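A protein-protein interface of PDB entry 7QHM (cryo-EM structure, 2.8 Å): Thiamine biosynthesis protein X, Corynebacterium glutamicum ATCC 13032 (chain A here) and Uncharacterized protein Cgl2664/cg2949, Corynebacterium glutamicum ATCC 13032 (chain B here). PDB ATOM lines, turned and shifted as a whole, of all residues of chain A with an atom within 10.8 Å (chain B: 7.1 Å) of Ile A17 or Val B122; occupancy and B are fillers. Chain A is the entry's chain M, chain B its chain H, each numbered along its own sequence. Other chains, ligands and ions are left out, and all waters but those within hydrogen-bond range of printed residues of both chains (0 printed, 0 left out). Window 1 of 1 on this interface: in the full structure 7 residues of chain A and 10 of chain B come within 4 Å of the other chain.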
ATOM      1  N   ARG A  13      27.163  38.018  28.048  1.00  0.00           N
ATOM      2  CA  ARG A  13      26.925  36.878  27.173  1.00  0.00           C
ATOM      3  C   ARG A  13      25.925  35.913  27.798  1.00  0.00           C
ATOM      4  O   ARG A  13      25.681  35.924  29.006  1.00  0.00           O
ATOM      5  CB  ARG A  13      28.233  36.127  26.854  1.00  0.00           C
ATOM      6  CG  ARG A  13      28.890  35.387  28.030  1.00  0.00           C
ATOM      7  CD  ARG A  13      30.086  34.573  27.559  1.00  0.00           C
ATOM      8  NE  ARG A  13      30.457  33.534  28.515  1.00  0.00           N
ATOM      9  CZ  ARG A  13      29.836  32.368  28.650  1.00  0.00           C
ATOM     10  NH1 ARG A  13      28.777  32.052  27.921  1.00  0.00           N
ATOM     11  NH2 ARG A  13      30.287  31.496  29.548  1.00  0.00           N
ATOM     12  N   THR A  14      25.353  35.074  26.936  1.00  0.00           N
ATOM     13  CA  THR A  14      24.608  33.895  27.348  1.00  0.00           C
ATOM     14  C   THR A  14      25.036  32.739  26.453  1.00  0.00           C
ATOM     15  O   THR A  14      25.578  32.941  25.364  1.00  0.00           O
ATOM     16  CB  THR A  14      23.086  34.115  27.289  1.00  0.00           C
ATOM     17  OG1 THR A  14      22.412  32.961  27.808  1.00  0.00           O
ATOM     18  CG2 THR A  14      22.611  34.382  25.860  1.00  0.00           C
ATOM     19  N   ASN A  15      24.784  31.522  26.924  1.00  0.00           N
ATOM     20  CA  ASN A  15      25.391  30.346  26.320  1.00  0.00           C
ATOM     21  C   ASN A  15      24.812  30.065  24.935  1.00  0.00           C
ATOM     22  O   ASN A  15      23.726  30.528  24.573  1.00  0.00           O
ATOM     23  CB  ASN A  15      25.203  29.132  27.228  1.00  0.00           C
ATOM     24  CG  ASN A  15      25.825  29.332  28.600  1.00  0.00           C
ATOM     25  OD1 ASN A  15      26.921  29.878  28.723  1.00  0.00           O
ATOM     26  ND2 ASN A  15      25.123  28.896  29.638  1.00  0.00           N
ATOM     27  N   GLU A  16      25.566  29.288  24.157  1.00  0.00           N
ATOM     28  CA  GLU A  16      25.229  28.969  22.776  1.00  0.00           C
ATOM     29  C   GLU A  16      25.582  27.513  22.502  1.00  0.00           C
ATOM     30  O   GLU A  16      26.413  26.915  23.190  1.00  0.00           O
ATOM     31  CB  GLU A  16      25.968  29.887  21.794  1.00  0.00           C
ATOM     32  CG  GLU A  16      27.481  29.727  21.828  1.00  0.00           C
ATOM     33  CD  GLU A  16      28.214  30.922  21.257  1.00  0.00           C
ATOM     34  OE1 GLU A  16      27.580  31.725  20.541  1.00  0.00           O
ATOM     35  OE2 GLU A  16      29.425  31.062  21.530  1.00  0.00           O
ATOM     36  N   ILE A  17      24.952  26.954  21.476  1.00  0.00           N
ATOM     37  CA  ILE A  17      25.072  25.536  21.157  1.00  0.00           C
ATOM     38  C   ILE A  17      26.275  25.330  20.247  1.00  0.00           C
ATOM     39  O   ILE A  17      26.639  26.203  19.452  1.00  0.00           O
ATOM     40  CB  ILE A  17      23.768  25.011  20.514  1.00  0.00           C
ATOM     41  CG1 ILE A  17      22.575  25.277  21.441  1.00  0.00           C
ATOM     42  CG2 ILE A  17      23.865  23.513  20.197  1.00  0.00           C
ATOM     43  CD1 ILE A  17      21.787  26.529  21.103  1.00  0.00           C
ATOM     44  N   LEU A  18      26.906  24.163  20.374  1.00  0.00           N
ATOM     45  CA  LEU A  18      27.970  23.724  19.483  1.00  0.00           C
ATOM     46  C   LEU A  18      27.677  22.290  19.056  1.00  0.00           C
ATOM     47  O   LEU A  18      26.856  21.603  19.672  1.00  0.00           O
ATOM     48  CB  LEU A  18      29.353  23.861  20.158  1.00  0.00           C
ATOM     49  CG  LEU A  18      29.643  23.152  21.489  1.00  0.00           C
ATOM     50  CD1 LEU A  18      29.992  21.695  21.281  1.00  0.00           C
ATOM     51  CD2 LEU A  18      30.764  23.866  22.244  1.00  0.00           C
ATOM     52  N   THR A  19      28.352  21.835  17.995  1.00  0.00           N
ATOM     53  CA  THR A  19      28.008  20.577  17.338  1.00  0.00           C
ATOM     54  C   THR A  19      29.262  19.786  16.984  1.00  0.00           C
ATOM     55  O   THR A  19      30.325  20.358  16.733  1.00  0.00           O
ATOM     56  CB  THR A  19      27.181  20.819  16.065  1.00  0.00           C
ATOM     57  OG1 THR A  19      27.935  21.615  15.143  1.00  0.00           O
ATOM     58  CG2 THR A  19      25.879  21.531  16.397  1.00  0.00           C
ATOM     59  N   THR A  20      29.117  18.461  16.949  1.00  0.00           N
ATOM     60  CA  THR A  20      30.230  17.554  16.684  1.00  0.00           C
ATOM     61  C   THR A  20      30.378  17.190  15.210  1.00  0.00           C
ATOM     62  O   THR A  20      31.314  16.459  14.870  1.00  0.00           O
ATOM     63  CB  THR A  20      30.083  16.260  17.515  1.00  0.00           C
ATOM     64  OG1 THR A  20      31.289  15.484  17.433  1.00  0.00           O
ATOM     65  CG2 THR A  20      28.895  15.405  17.054  1.00  0.00           C
ATOM     66  N   SER A  21      29.492  17.666  14.333  1.00  0.00           N
ATOM     67  CA  SER A  21      29.490  17.286  12.919  1.00  0.00           C
ATOM     68  C   SER A  21      29.346  15.767  12.776  1.00  0.00           C
ATOM     69  O   SER A  21      30.268  15.050  12.384  1.00  0.00           O
ATOM     70  CB  SER A  21      30.757  17.785  12.211  1.00  0.00           C
ATOM     71  OG  SER A  21      30.899  19.189  12.335  1.00  0.00           O
ATOM     72  N   THR B  34      19.914  17.263  32.680  1.00  0.00           N
ATOM     73  CA  THR B  34      21.056  17.182  31.782  1.00  0.00           C
ATOM     74  C   THR B  34      20.659  16.392  30.547  1.00  0.00           C
ATOM     75  O   THR B  34      19.681  15.643  30.555  1.00  0.00           O
ATOM     76  CB  THR B  34      22.285  16.547  32.452  1.00  0.00           C
ATOM     77  OG1 THR B  34      23.302  16.319  31.469  1.00  0.00           O
ATOM     78  CG2 THR B  34      21.947  15.237  33.127  1.00  0.00           C
ATOM     79  N   VAL B  35      21.418  16.588  29.473  1.00  0.00           N
ATOM     80  CA  VAL B  35      21.218  15.877  28.218  1.00  0.00           C
ATOM     81  C   VAL B  35      22.269  14.778  28.167  1.00  0.00           C
ATOM     82  O   VAL B  35      23.406  15.007  27.755  1.00  0.00           O
ATOM     83  CB  VAL B  35      21.310  16.807  27.008  1.00  0.00           C
ATOM     84  CG1 VAL B  35      21.407  15.994  25.709  1.00  0.00           C
ATOM     85  CG2 VAL B  35      20.099  17.735  26.966  1.00  0.00           C
ATOM     86  N   VAL B  66      14.503  20.199  23.187  1.00  0.00           N
ATOM     87  CA  VAL B  66      15.923  20.397  23.432  1.00  0.00           C
ATOM     88  C   VAL B  66      16.490  21.109  22.210  1.00  0.00           C
ATOM     89  O   VAL B  66      16.661  20.497  21.148  1.00  0.00           O
ATOM     90  CB  VAL B  66      16.639  19.053  23.682  1.00  0.00           C
ATOM     91  CG1 VAL B  66      18.094  19.267  24.051  1.00  0.00           C
ATOM     92  CG2 VAL B  66      15.934  18.249  24.768  1.00  0.00           C
ATOM     93  N   ASP B  67      16.762  22.409  22.347  1.00  0.00           N
ATOM     94  CA  ASP B  67      17.248  23.246  21.247  1.00  0.00           C
ATOM     95  C   ASP B  67      16.342  23.126  20.024  1.00  0.00           C
ATOM     96  O   ASP B  67      16.800  23.037  18.883  1.00  0.00           O
ATOM     97  CB  ASP B  67      18.695  22.898  20.889  1.00  0.00           C
ATOM     98  CG  ASP B  67      19.339  23.931  19.976  1.00  0.00           C
ATOM     99  OD1 ASP B  67      18.751  25.017  19.785  1.00  0.00           O
ATOM    100  OD2 ASP B  67      20.429  23.650  19.435  1.00  0.00           O
ATOM    101  N   PRO B 114      20.721  15.324  17.757  1.00  0.00           N
ATOM    102  CA  PRO B 114      20.912  16.209  16.601  1.00  0.00           C
ATOM    103  C   PRO B 114      22.321  16.785  16.519  1.00  0.00           C
ATOM    104  O   PRO B 114      22.502  17.964  16.201  1.00  0.00           O
ATOM    105  CB  PRO B 114      19.856  17.296  16.837  1.00  0.00           C
ATOM    106  CG  PRO B 114      19.822  17.423  18.306  1.00  0.00           C
ATOM    107  CD  PRO B 114      20.013  16.029  18.847  1.00  0.00           C
ATOM    108  N   GLY B 115      23.330  15.964  16.800  1.00  0.00           N
ATOM    109  CA  GLY B 115      24.705  16.388  16.638  1.00  0.00           C
ATOM    110  C   GLY B 115      25.289  17.186  17.781  1.00  0.00           C
ATOM    111  O   GLY B 115      26.203  17.981  17.556  1.00  0.00           O
ATOM    112  N   PHE B 116      24.799  16.998  19.005  1.00  0.00           N
ATOM    113  CA  PHE B 116      25.386  17.686  20.144  1.00  0.00           C
ATOM    114  C   PHE B 116      26.801  17.186  20.394  1.00  0.00           C
ATOM    115  O   PHE B 116      27.264  16.211  19.795  1.00  0.00           O
ATOM    116  CB  PHE B 116      24.555  17.475  21.410  1.00  0.00           C
ATOM    117  CG  PHE B 116      23.166  18.035  21.344  1.00  0.00           C
ATOM    118  CD1 PHE B 116      22.897  19.222  20.684  1.00  0.00           C
ATOM    119  CD2 PHE B 116      22.125  17.370  21.958  1.00  0.00           C
ATOM    120  CE1 PHE B 116      21.620  19.728  20.630  1.00  0.00           C
ATOM    121  CE2 PHE B 116      20.844  17.869  21.910  1.00  0.00           C
ATOM    122  CZ  PHE B 116      20.590  19.054  21.249  1.00  0.00           C
ATOM    123  N   ALA B 117      27.494  17.876  21.297  1.00  0.00           N
ATOM    124  CA  ALA B 117      28.832  17.479  21.699  1.00  0.00           C
ATOM    125  C   ALA B 117      29.041  17.870  23.150  1.00  0.00           C
ATOM    126  O   ALA B 117      28.430  18.817  23.650  1.00  0.00           O
ATOM    127  CB  ALA B 117      29.916  18.117  20.826  1.00  0.00           C
ATOM    128  N   GLY B 120      29.451  21.576  26.198  1.00  0.00           N
ATOM    129  CA  GLY B 120      28.570  22.705  26.022  1.00  0.00           C
ATOM    130  C   GLY B 120      27.262  22.522  26.764  1.00  0.00           C
ATOM    131  O   GLY B 120      27.082  21.624  27.586  1.00  0.00           O
ATOM    132  N   VAL B 121      26.322  23.415  26.456  1.00  0.00           N
ATOM    133  CA  VAL B 121      24.989  23.389  27.036  1.00  0.00           C
ATOM    134  C   VAL B 121      23.976  23.677  25.938  1.00  0.00           C
ATOM    135  O   VAL B 121      24.304  24.227  24.885  1.00  0.00           O
ATOM    136  CB  VAL B 121      24.821  24.395  28.200  1.00  0.00           C
ATOM    137  CG1 VAL B 121      25.822  24.110  29.304  1.00  0.00           C
ATOM    138  CG2 VAL B 121      24.975  25.830  27.712  1.00  0.00           C
ATOM    139  N   VAL B 122      22.733  23.284  26.201  1.00  0.00           N
ATOM    140  CA  VAL B 122      21.624  23.470  25.273  1.00  0.00           C
ATOM    141  C   VAL B 122      20.400  23.909  26.073  1.00  0.00           C
ATOM    142  O   VAL B 122      20.188  23.397  27.180  1.00  0.00           O
ATOM    143  CB  VAL B 122      21.337  22.188  24.474  1.00  0.00           C
ATOM    144  CG1 VAL B 122      22.479  21.896  23.515  1.00  0.00           C
ATOM    145  CG2 VAL B 122      21.104  20.993  25.398  1.00  0.00           C
ATOM    146  N   PRO B 123      19.574  24.834  25.587  1.00  0.00           N
ATOM    147  CA  PRO B 123      18.338  25.147  26.310  1.00  0.00           C
ATOM    148  C   PRO B 123      17.283  24.072  26.106  1.00  0.00           C
ATOM    149  O   PRO B 123      17.091  23.566  24.997  1.00  0.00           O
ATOM    150  CB  PRO B 123      17.901  26.480  25.695  1.00  0.00           C
ATOM    151  CG  PRO B 123      18.424  26.426  24.319  1.00  0.00           C
ATOM    152  CD  PRO B 123      19.723  25.684  24.393  1.00  0.00           C
ATOM    153  N   VAL B 124      16.591  23.733  27.191  1.00  0.00           N
ATOM    154  CA  VAL B 124      15.549  22.716  27.217  1.00  0.00           C
ATOM    155  C   VAL B 124      14.273  23.390  27.695  1.00  0.00           C
ATOM    156  O   VAL B 124      14.322  24.367  28.448  1.00  0.00           O
ATOM    157  CB  VAL B 124      15.942  21.540  28.142  1.00  0.00           C
ATOM    158  CG1 VAL B 124      14.899  20.440  28.129  1.00  0.00           C
ATOM    159  CG2 VAL B 124      17.292  20.984  27.744  1.00  0.00           C
ATOM    160  N   GLU B 125      13.130  22.878  27.244  1.00  0.00           N
ATOM    161  CA  GLU B 125      11.834  23.413  27.636  1.00  0.00           C
ATOM    162  C   GLU B 125      10.871  22.275  27.930  1.00  0.00           C
ATOM    163  O   GLU B 125      10.815  21.287  27.191  1.00  0.00           O
ATOM    164  CB  GLU B 125      11.258  24.333  26.557  1.00  0.00           C
ATOM    165  CG  GLU B 125       9.981  25.033  26.986  1.00  0.00           C
ATOM    166  CD  GLU B 125       9.769  26.363  26.288  1.00  0.00           C
ATOM    167  OE1 GLU B 125      10.376  26.591  25.221  1.00  0.00           O
ATOM    168  OE2 GLU B 125       8.992  27.187  26.816  1.00  0.00           O
ATOM    169  N   ILE B 135      15.037  25.693  30.905  1.00  0.00           N
ATOM    170  CA  ILE B 135      16.243  25.587  31.711  1.00  0.00           C
ATOM    171  C   ILE B 135      17.376  25.137  30.805  1.00  0.00           C
ATOM    172  O   ILE B 135      17.189  24.295  29.929  1.00  0.00           O
ATOM    173  CB  ILE B 135      16.037  24.614  32.898  1.00  0.00           C
ATOM    174  CG1 ILE B 135      17.374  24.323  33.587  1.00  0.00           C
ATOM    175  CG2 ILE B 135      15.375  23.318  32.437  1.00  0.00           C
ATOM    176  CD1 ILE B 135      17.231  23.730  34.941  1.00  0.00           C
ATOM    177  N   ASP B 136      18.556  25.705  31.025  1.00  0.00           N
ATOM    178  CA  ASP B 136      19.740  25.321  30.273  1.00  0.00           C
ATOM    179  C   ASP B 136      20.325  24.048  30.872  1.00  0.00           C
ATOM    180  O   ASP B 136      20.445  23.934  32.094  1.00  0.00           O
ATOM    181  CB  ASP B 136      20.757  26.460  30.310  1.00  0.00           C
ATOM    182  CG  ASP B 136      21.810  26.356  29.229  1.00  0.00           C
ATOM    183  OD1 ASP B 136      21.720  25.457  28.368  1.00  0.00           O
ATOM    184  OD2 ASP B 136      22.739  27.188  29.242  1.00  0.00           O
ATOM    185  N   ALA B 137      20.692  23.091  30.016  1.00  0.00           N
ATOM    186  CA  ALA B 137      21.143  21.773  30.439  1.00  0.00           C
ATOM    187  C   ALA B 137      22.433  21.412  29.721  1.00  0.00           C
ATOM    188  O   ALA B 137      22.548  21.612  28.511  1.00  0.00           O
ATOM    189  CB  ALA B 137      20.081  20.718  30.138  1.00  0.00           C
ATOM    190  N   THR B 138      23.396  20.869  30.456  1.00  0.00           N
ATOM    191  CA  THR B 138      24.670  20.516  29.849  1.00  0.00           C
ATOM    192  C   THR B 138      24.593  19.144  29.201  1.00  0.00           C
ATOM    193  O   THR B 138      23.876  18.252  29.660  1.00  0.00           O
ATOM    194  CB  THR B 138      25.812  20.552  30.874  1.00  0.00           C
ATOM    195  OG1 THR B 138      27.063  20.370  30.204  1.00  0.00           O
ATOM    196  CG2 THR B 138      25.666  19.475  31.944  1.00  0.00           C
ATOM    197  N   VAL B 139      25.330  18.992  28.110  1.00  0.00           N
ATOM    198  CA  VAL B 139      25.523  17.687  27.496  1.00  0.00           C
ATOM    199  C   VAL B 139      26.617  16.973  28.272  1.00  0.00           C
ATOM    200  O   VAL B 139      27.680  17.547  28.534  1.00  0.00           O
ATOM    201  CB  VAL B 139      25.881  17.827  26.008  1.00  0.00           C
ATOM    202  CG1 VAL B 139      25.982  16.464  25.337  1.00  0.00           C
ATOM    203  CG2 VAL B 139      24.852  18.693  25.292  1.00  0.00           C
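OD2 of Asp B136 lies within hydrogen-bond range of ND2 of Asn A15 (3.0 Å). The backbone carbonyl oxygen (O) of Gly B115 lies within hydrogen-bond range of the backbone NH (N) of Thr A20 (3.0 Å).
The side-chain amide oxygen (OD1) of Asn A15 sits at hydrogen-bond distance from the guanidinium group (NH1) of Arg A13, at 3.0 Å. The backbone NH (N) of Asp B67 is in hydrogen-bond range of the backbone carbonyl oxygen (O) of Pro B123. The side-chain carboxylate (OD1) of Asp B136 sits close to the backbone NH (N) of Val B122, at 3.2 Å. O of Ala B137 sits at hydrogen-bond distance from N of Val B122, 2.9 Å away.
Among the printed residues, merely in contact across the chains: Thr A19 with Gly B115, Thr A20 with Phe B116, Asn A15 with Val B121, Ile A17 with Asp B67, Leu A18 with Ala B117, Thr A20 with Ala B117, Glu A16 with Val B121, Ile A17 with Val B122, Ile A17 with Pro B123 and Ile A17 with Val B121.
Of the printed residues of chain B, Glu A16 touches Val B121 (3.8 Å). Printed residues of chain B within 4 Å of Ile A17: Asp B67, Val B121, Val B122 and Pro B123. Of the printed residues of chain B, Thr A19 touches Gly B115 (3.2 Å). Asp B67 touches just one residue of chain A: Ile A17. Of chain A, only Ile A17 comes within 4 Å of Val B122. Pro B123 touches just one residue of chain A: Ile A17 (3.97 Å). No residue of chain A comes within 4 Å of Val B124. Asp B136 touches just one residue of chain A: Asn A15 (3.0 Å). No residue of chain A comes within 4 Å of Ala B137. Thr B138 touches none of the printed residues of chain A. The nearest printed residue of chain B that does not touch Ile A17 is Phe B116 (4.4 Å). The nearest residue of chain A that does not touch Val B122 is Leu A18 (5.8 Å).
Printed residues of chain B that touch a printed residue of chain A: Asp B67, Gly B115, Phe B116, Ala B117, Val B121, Val B122, Pro B123 and Asp B136. Hydrophobic or aromatic side chains of chain B that line the printed part of chain A: Ala B117, Val B121, Val B122 and Pro B123. Printed residues of chain A that touch a printed residue of chain B: Asn A15, Glu A16, Ile A17, Leu A18, Thr A19 and Thr A20. Among the printed residues, 12 pairs touch across the chains.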
